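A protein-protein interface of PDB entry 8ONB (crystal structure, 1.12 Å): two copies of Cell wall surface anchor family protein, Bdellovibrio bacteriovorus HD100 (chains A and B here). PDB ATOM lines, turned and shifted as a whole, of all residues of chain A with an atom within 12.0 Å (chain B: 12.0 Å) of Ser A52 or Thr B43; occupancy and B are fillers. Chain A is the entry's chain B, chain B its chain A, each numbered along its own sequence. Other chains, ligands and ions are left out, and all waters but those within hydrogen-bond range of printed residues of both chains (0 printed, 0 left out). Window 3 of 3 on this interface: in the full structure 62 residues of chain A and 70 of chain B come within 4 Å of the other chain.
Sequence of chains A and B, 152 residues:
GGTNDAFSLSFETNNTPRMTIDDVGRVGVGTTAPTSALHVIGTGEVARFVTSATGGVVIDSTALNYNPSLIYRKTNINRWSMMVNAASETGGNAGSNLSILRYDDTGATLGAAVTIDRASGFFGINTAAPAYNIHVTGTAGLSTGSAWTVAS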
ATOM      1  N   ARG A  48      29.806 -31.067 -18.001  1.00  0.00           N
ATOM      2  CA  ARG A  48      29.438 -29.788 -17.331  1.00  0.00           C
ATOM      3  C   ARG A  48      28.485 -30.116 -16.175  1.00  0.00           C
ATOM      4  O   ARG A  48      27.392 -30.650 -16.439  1.00  0.00           O
ATOM      5  CB  ARG A  48      28.921 -28.752 -18.338  1.00  0.00           C
ATOM      6  CG  ARG A  48      28.807 -27.341 -17.773  1.00  0.00           C
ATOM      7  CD  ARG A  48      28.637 -26.250 -18.816  1.00  0.00           C
ATOM      8  NE  ARG A  48      27.545 -26.477 -19.748  1.00  0.00           N
ATOM      9  CZ  ARG A  48      26.381 -25.841 -19.716  1.00  0.00           C
ATOM     10  NH1 ARG A  48      26.156 -24.922 -18.793  1.00  0.00           N
ATOM     11  NH2 ARG A  48      25.451 -26.117 -20.612  1.00  0.00           N
ATOM     12  N   PHE A  49      28.824 -29.638 -14.975  1.00  0.00           N
ATOM     13  CA  PHE A  49      28.061 -29.870 -13.756  1.00  0.00           C
ATOM     14  C   PHE A  49      27.543 -28.505 -13.343  1.00  0.00           C
ATOM     15  O   PHE A  49      28.346 -27.607 -13.065  1.00  0.00           O
ATOM     16  CB  PHE A  49      28.986 -30.454 -12.678  1.00  0.00           C
ATOM     17  CG  PHE A  49      29.586 -31.786 -13.071  1.00  0.00           C
ATOM     18  CD1 PHE A  49      28.920 -32.958 -12.788  1.00  0.00           C
ATOM     19  CD2 PHE A  49      30.800 -31.858 -13.747  1.00  0.00           C
ATOM     20  CE1 PHE A  49      29.431 -34.180 -13.180  1.00  0.00           C
ATOM     21  CE2 PHE A  49      31.319 -33.113 -14.143  1.00  0.00           C
ATOM     22  CZ  PHE A  49      30.633 -34.259 -13.855  1.00  0.00           C
ATOM     23  N   VAL A  50      26.232 -28.335 -13.306  1.00  0.00           N
ATOM     24  CA  VAL A  50      25.628 -27.017 -13.122  1.00  0.00           C
ATOM     25  C   VAL A  50      24.847 -27.018 -11.826  1.00  0.00           C
ATOM     26  O   VAL A  50      23.932 -27.822 -11.658  1.00  0.00           O
ATOM     27  CB  VAL A  50      24.722 -26.614 -14.294  1.00  0.00           C
ATOM     28  CG1 VAL A  50      24.231 -25.173 -14.113  1.00  0.00           C
ATOM     29  CG2 VAL A  50      25.430 -26.810 -15.623  1.00  0.00           C
ATOM     30  N   THR A  51      25.157 -26.082 -10.937  1.00  0.00           N
ATOM     31  CA  THR A  51      24.474 -25.994  -9.660  1.00  0.00           C
ATOM     32  C   THR A  51      23.625 -24.732  -9.583  1.00  0.00           C
ATOM     33  O   THR A  51      24.051 -23.648 -10.006  1.00  0.00           O
ATOM     34  CB  THR A  51      25.469 -26.056  -8.497  1.00  0.00           C
ATOM     35  OG1 THR A  51      24.736 -25.959  -7.263  1.00  0.00           O
ATOM     36  CG2 THR A  51      26.542 -24.951  -8.587  1.00  0.00           C
ATOM     37  N   SER A  52      22.418 -24.885  -9.031  1.00  0.00           N
ATOM     38  CA  SER A  52      21.472 -23.797  -8.805  1.00  0.00           C
ATOM     39  C   SER A  52      21.514 -23.305  -7.371  1.00  0.00           C
ATOM     40  O   SER A  52      20.522 -22.763  -6.866  1.00  0.00           O
ATOM     41  CB  SER A  52      20.057 -24.234  -9.176  1.00  0.00           C
ATOM     42  OG  SER A  52      19.664 -25.345  -8.394  1.00  0.00           O
ATOM     43  N   ALA A  53      22.632 -23.535  -6.698  1.00  0.00           N
ATOM     44  CA  ALA A  53      22.959 -22.938  -5.415  1.00  0.00           C
ATOM     45  C   ALA A  53      24.470 -23.022  -5.339  1.00  0.00           C
ATOM     46  O   ALA A  53      25.100 -23.638  -6.194  1.00  0.00           O
ATOM     47  CB  ALA A  53      22.319 -23.724  -4.265  1.00  0.00           C
ATOM     48  N   THR A  54      25.057 -22.419  -4.315  1.00  0.00           N
ATOM     49  CA  THR A  54      26.480 -22.662  -4.102  1.00  0.00           C
ATOM     50  C   THR A  54      26.696 -24.162  -3.909  1.00  0.00           C
ATOM     51  O   THR A  54      25.907 -24.837  -3.246  1.00  0.00           O
ATOM     52  CB  THR A  54      26.961 -21.872  -2.893  1.00  0.00           C
ATOM     53  OG1 THR A  54      26.974 -20.482  -3.236  1.00  0.00           O
ATOM     54  CG2 THR A  54      28.362 -22.304  -2.461  1.00  0.00           C
ATOM     55  N   GLY A  55      27.726 -24.700  -4.540  1.00  0.00           N
ATOM     56  CA  GLY A  55      27.926 -26.137  -4.553  1.00  0.00           C
ATOM     57  C   GLY A  55      28.692 -26.518  -5.797  1.00  0.00           C
ATOM     58  O   GLY A  55      29.381 -25.682  -6.368  1.00  0.00           O
ATOM     59  N   GLY A  56      28.531 -27.776  -6.219  1.00  0.00           N
ATOM     60  CA  GLY A  56      29.233 -28.266  -7.381  1.00  0.00           C
ATOM     61  C   GLY A  56      29.500 -29.757  -7.298  1.00  0.00           C
ATOM     62  O   GLY A  56      28.561 -30.566  -7.143  1.00  0.00           O
ATOM     63  N   VAL A  57      30.767 -30.134  -7.432  1.00  0.00           N
ATOM     64  CA  VAL A  57      31.177 -31.524  -7.538  1.00  0.00           C
ATOM     65  C   VAL A  57      31.880 -31.905  -6.250  1.00  0.00           C
ATOM     66  O   VAL A  57      32.720 -31.137  -5.755  1.00  0.00           O
ATOM     67  CB  VAL A  57      32.128 -31.695  -8.732  1.00  0.00           C
ATOM     68  CG1 VAL A  57      32.802 -33.086  -8.731  1.00  0.00           C
ATOM     69  CG2 VAL A  57      31.409 -31.372 -10.048  1.00  0.00           C
ATOM     70  N   VAL A  58      31.592 -33.107  -5.752  1.00  0.00           N
ATOM     71  CA  VAL A  58      32.236 -33.681  -4.570  1.00  0.00           C
ATOM     72  C   VAL A  58      33.117 -34.857  -4.977  1.00  0.00           C
ATOM     73  O   VAL A  58      32.665 -35.741  -5.719  1.00  0.00           O
ATOM     74  CB  VAL A  58      31.203 -34.135  -3.534  1.00  0.00           C
ATOM     75  CG1 VAL A  58      31.889 -34.820  -2.352  1.00  0.00           C
ATOM     76  CG2 VAL A  58      30.298 -32.980  -3.077  1.00  0.00           C
ATOM     77  N   HIS B  39      26.108 -33.791 -19.077  1.00  0.00           N
ATOM     78  CA  HIS B  39      25.613 -32.521 -18.552  1.00  0.00           C
ATOM     79  C   HIS B  39      24.727 -32.862 -17.366  1.00  0.00           C
ATOM     80  O   HIS B  39      23.714 -33.536 -17.532  1.00  0.00           O
ATOM     81  CB  HIS B  39      24.874 -31.805 -19.665  1.00  0.00           C
ATOM     82  CG  HIS B  39      24.370 -30.457 -19.277  1.00  0.00           C
ATOM     83  ND1 HIS B  39      24.069 -29.486 -20.204  1.00  0.00           N
ATOM     84  CD2 HIS B  39      24.088 -29.917 -18.067  1.00  0.00           C
ATOM     85  CE1 HIS B  39      23.637 -28.399 -19.586  1.00  0.00           C
ATOM     86  NE2 HIS B  39      23.632 -28.635 -18.287  1.00  0.00           N
ATOM     87  N   VAL B  40      25.167 -32.505 -16.160  1.00  0.00           N
ATOM     88  CA  VAL B  40      24.465 -32.834 -14.927  1.00  0.00           C
ATOM     89  C   VAL B  40      23.984 -31.542 -14.309  1.00  0.00           C
ATOM     90  O   VAL B  40      24.774 -30.600 -14.165  1.00  0.00           O
ATOM     91  CB  VAL B  40      25.363 -33.592 -13.938  1.00  0.00           C
ATOM     92  CG1 VAL B  40      24.534 -34.059 -12.737  1.00  0.00           C
ATOM     93  CG2 VAL B  40      26.080 -34.752 -14.630  1.00  0.00           C
ATOM     94  N   ILE B  41      22.718 -31.500 -13.912  1.00  0.00           N
ATOM     95  CA  ILE B  41      22.172 -30.340 -13.228  1.00  0.00           C
ATOM     96  C   ILE B  41      21.701 -30.770 -11.851  1.00  0.00           C
ATOM     97  O   ILE B  41      21.128 -31.856 -11.686  1.00  0.00           O
ATOM     98  CB  ILE B  41      21.065 -29.625 -14.028  1.00  0.00           C
ATOM     99  CG1 ILE B  41      19.860 -30.540 -14.214  1.00  0.00           C
ATOM    100  CG2 ILE B  41      21.591 -29.177 -15.394  1.00  0.00           C
ATOM    101  CD1 ILE B  41      18.573 -29.803 -14.540  1.00  0.00           C
ATOM    102  N   GLY B  42      21.918 -29.907 -10.872  1.00  0.00           N
ATOM    103  CA  GLY B  42      21.420 -30.163  -9.536  1.00  0.00           C
ATOM    104  C   GLY B  42      21.465 -28.893  -8.720  1.00  0.00           C
ATOM    105  O   GLY B  42      21.706 -27.803  -9.243  1.00  0.00           O
ATOM    106  N   THR B  43      21.202 -29.040  -7.430  1.00  0.00           N
ATOM    107  CA  THR B  43      21.210 -27.919  -6.493  1.00  0.00           C
ATOM    108  C   THR B  43      22.143 -28.277  -5.348  1.00  0.00           C
ATOM    109  O   THR B  43      21.825 -29.152  -4.535  1.00  0.00           O
ATOM    110  CB  THR B  43      19.807 -27.638  -5.964  1.00  0.00           C
ATOM    111  OG1 THR B  43      18.911 -27.482  -7.068  1.00  0.00           O
ATOM    112  CG2 THR B  43      19.803 -26.357  -5.112  1.00  0.00           C
ATOM    113  N   GLY B  44      23.280 -27.590  -5.264  1.00  0.00           N
ATOM    114  CA  GLY B  44      24.250 -27.886  -4.232  1.00  0.00           C
ATOM    115  C   GLY B  44      25.179 -28.999  -4.659  1.00  0.00           C
ATOM    116  O   GLY B  44      26.052 -28.792  -5.502  1.00  0.00           O
ATOM    117  N   GLU B  45      24.983 -30.198  -4.126  1.00  0.00           N
ATOM    118  CA  GLU B  45      25.812 -31.351  -4.477  1.00  0.00           C
ATOM    119  C   GLU B  45      25.273 -31.931  -5.779  1.00  0.00           C
ATOM    120  O   GLU B  45      24.300 -32.687  -5.784  1.00  0.00           O
ATOM    121  CB  GLU B  45      25.751 -32.372  -3.350  1.00  0.00           C
ATOM    122  CG  GLU B  45      26.713 -33.535  -3.486  1.00  0.00           C
ATOM    123  CD  GLU B  45      26.685 -34.421  -2.258  1.00  0.00           C
ATOM    124  OE1 GLU B  45      26.496 -33.873  -1.152  1.00  0.00           O
ATOM    125  OE2 GLU B  45      26.833 -35.655  -2.397  1.00  0.00           O
ATOM    126  N   VAL B  46      25.887 -31.560  -6.898  1.00  0.00           N
ATOM    127  CA  VAL B  46      25.426 -32.001  -8.211  1.00  0.00           C
ATOM    128  C   VAL B  46      25.871 -33.435  -8.496  1.00  0.00           C
ATOM    129  O   VAL B  46      25.106 -34.244  -9.051  1.00  0.00           O
ATOM    130  CB  VAL B  46      25.976 -31.009  -9.257  1.00  0.00           C
ATOM    131  CG1 VAL B  46      25.632 -31.449 -10.650  1.00  0.00           C
ATOM    132  CG2 VAL B  46      25.446 -29.598  -8.984  1.00  0.00           C
ATOM    133  N   ALA B  47      27.119 -33.750  -8.183  1.00  0.00           N
ATOM    134  CA  ALA B  47      27.668 -35.059  -8.454  1.00  0.00           C
ATOM    135  C   ALA B  47      28.673 -35.386  -7.371  1.00  0.00           C
ATOM    136  O   ALA B  47      29.319 -34.487  -6.812  1.00  0.00           O
ATOM    137  CB  ALA B  47      28.339 -35.110  -9.821  1.00  0.00           C
ATOM    138  N   ARG B  48      28.788 -36.669  -7.062  1.00  0.00           N
ATOM    139  CA  ARG B  48      29.725 -37.159  -6.076  1.00  0.00           C
ATOM    140  C   ARG B  48      30.442 -38.357  -6.657  1.00  0.00           C
ATOM    141  O   ARG B  48      29.798 -39.293  -7.130  1.00  0.00           O
ATOM    142  CB  ARG B  48      29.022 -37.539  -4.763  1.00  0.00           C
ATOM    143  CG  ARG B  48      29.986 -37.945  -3.639  1.00  0.00           C
ATOM    144  CD  ARG B  48      29.549 -37.395  -2.278  1.00  0.00           C
ATOM    145  NE  ARG B  48      28.247 -37.903  -1.862  1.00  0.00           N
ATOM    146  CZ  ARG B  48      28.081 -38.989  -1.118  1.00  0.00           C
ATOM    147  NH1 ARG B  48      29.139 -39.679  -0.699  1.00  0.00           N
ATOM    148  NH2 ARG B  48      26.856 -39.381  -0.792  1.00  0.00           N
ATOM    149  N   ARG B  73      32.842 -21.698 -13.959  1.00  0.00           N
ATOM    150  CA  ARG B  73      32.039 -20.670 -14.598  1.00  0.00           C
ATOM    151  C   ARG B  73      30.920 -20.234 -13.673  1.00  0.00           C
ATOM    152  O   ARG B  73      30.483 -21.004 -12.806  1.00  0.00           O
ATOM    153  CB  ARG B  73      31.406 -21.196 -15.894  1.00  0.00           C
ATOM    154  CG  ARG B  73      32.450 -21.567 -16.944  1.00  0.00           C
ATOM    155  CD  ARG B  73      31.792 -22.017 -18.252  1.00  0.00           C
ATOM    156  NE  ARG B  73      32.829 -22.324 -19.212  1.00  0.00           N
ATOM    157  CZ  ARG B  73      32.651 -23.092 -20.266  1.00  0.00           C
ATOM    158  NH1 ARG B  73      31.452 -23.630 -20.487  1.00  0.00           N
ATOM    159  NH2 ARG B  73      33.687 -23.350 -21.060  1.00  0.00           N
ATOM    160  N   LYS B  74      30.454 -19.001 -13.867  1.00  0.00           N
ATOM    161  CA  LYS B  74      29.199 -18.531 -13.295  1.00  0.00           C
ATOM    162  C   LYS B  74      28.329 -18.061 -14.444  1.00  0.00           C
ATOM    163  O   LYS B  74      28.777 -17.257 -15.263  1.00  0.00           O
ATOM    164  CB  LYS B  74      29.428 -17.379 -12.312  1.00  0.00           C
ATOM    165  CG  LYS B  74      29.991 -17.843 -10.990  1.00  0.00           C
ATOM    166  CD  LYS B  74      30.210 -16.668 -10.018  1.00  0.00           C
ATOM    167  CE  LYS B  74      30.423 -17.136  -8.586  1.00  0.00           C
ATOM    168  NZ  LYS B  74      30.489 -15.946  -7.685  1.00  0.00           N
ATOM    169  N   THR B  75      27.086 -18.521 -14.469  1.00  0.00           N
ATOM    170  CA  THR B  75      26.171 -18.275 -15.587  1.00  0.00           C
ATOM    171  C   THR B  75      26.822 -18.630 -16.924  1.00  0.00           C
ATOM    172  O   THR B  75      26.608 -17.973 -17.939  1.00  0.00           O
ATOM    173  CB  THR B  75      25.554 -16.860 -15.589  1.00  0.00           C
ATOM    174  OG1 THR B  75      26.563 -15.867 -15.814  1.00  0.00           O
ATOM    175  CG2 THR B  75      24.874 -16.571 -14.261  1.00  0.00           C
ATOM    176  N   ASN B  76      27.644 -19.685 -16.902  1.00  0.00           N
ATOM    177  CA  ASN B  76      28.325 -20.206 -18.087  1.00  0.00           C
ATOM    178  C   ASN B  76      29.336 -19.225 -18.675  1.00  0.00           C
ATOM    179  O   ASN B  76      29.633 -19.281 -19.875  1.00  0.00           O
ATOM    180  CB  ASN B  76      27.372 -20.777 -19.150  1.00  0.00           C
ATOM    181  CG  ASN B  76      28.018 -21.899 -19.959  1.00  0.00           C
ATOM    182  OD1 ASN B  76      28.892 -22.626 -19.460  1.00  0.00           O
ATOM    183  ND2 ASN B  76      27.607 -22.036 -21.212  1.00  0.00           N
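The backbone carbonyl oxygen (O) of Arg A48 sits at hydrogen-bond distance from the backbone NH (N) of Val B40 (2.9 Å).
O of Val B40 sits at hydrogen-bond distance from N of Val A50 (2.8 Å).
N of Gly B42 is in hydrogen-bond range of O of Val A50, at 3.0 Å.
The backbone carbonyl oxygen (O) of Gly B42 is in hydrogen-bond range of the backbone NH (N) of Ser A52, at 3.0 Å.
OG1 of Thr B43 is in hydrogen-bond range of OG of Ser A52.
The backbone NH (N) of Gly B44 lies within hydrogen-bond range of the side-chain hydroxyl (OG1) of Thr A51.
O of Gly B44 lies within hydrogen-bond range of N of Gly A56.
The backbone carbonyl oxygen (O) of Gly A56 sits at hydrogen-bond distance from the backbone NH (N) of Val B46 (2.9 Å).
N of Val A58 is in hydrogen-bond range of O of Ala B47 (2.9 Å).
NE of Arg B48 is in salt-bridge range of OE2 of Glu B45 (2.7 Å).
NH1 of Arg B73 lies within hydrogen-bond range of OD1 of Asn B76.
O of Ala A53 lies within hydrogen-bond range of OG1 of Thr A51, 2.6 Å away.
NH2 of Arg A48 touches CE1 of His B39 (3.1 Å).
Val B40 touches Phe A49.
CE1 of Phe A49 touches CB of Ala B47 (3.7 Å).
CA of Ile B41 touches O of Val A50 (3.5 Å).
O of Val A50 touches CG2 of Val B46 (3.5 Å).
CA of Thr A51 touches O of Gly B42, 3.3 Å away.
Thr A51 touches Thr B43.
Glu B45 touches Gly A56.
Val A58 touches Glu B45.
Arg B48 touches Val A58 (CA to O, 3.3 Å).
Printed residues of chain B within 4 Å of Ser A52: Gly B42 (3.0 Å) and Thr B43 (2.6 Å).
Thr B43 touches just these residues of chain A: Thr A51, Ser A52 and Ala A53.
Val A50 touches just these residues of chain B: His B39 (3.7 Å), Val B40 (2.8 Å), Ile B41 (3.5 Å), Gly B42 (3.0 Å) and Val B46 (3.5 Å).
Of chain B, only Gly B42 (3.3 Å), Thr B43 (3.97 Å), Gly B44 (3.0 Å) and Val B46 (3.6 Å) come within 4 Å of Thr A51.
Of chain B, only Gly B44, Glu B45, Val B46 and Ala B47 come within 4 Å of Gly A56.
Of chain A, only Val A50 (3.5 Å) comes within 4 Å of Ile B41.
Val B46 touches just these residues of chain A: Val A50 (3.5 Å), Thr A51 (3.6 Å) and Gly A56 (2.9 Å).
Of the printed residues of chain B, Arg A48 touches His B39, Val B40 and Asn B76.
Printed residues of chain A within 4 Å of Val B40: Arg A48 (2.9 Å), Phe A49 (3.4 Å) and Val A50 (2.8 Å).
Arg B73 touches none of the printed residues of chain A.
Of the 11 printed residues of chain A, 11 touch a printed residue of chain B.
Of the 14 printed residues of chain B, 11 touch a printed residue of chain A.
Position printed for both chains: 48.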
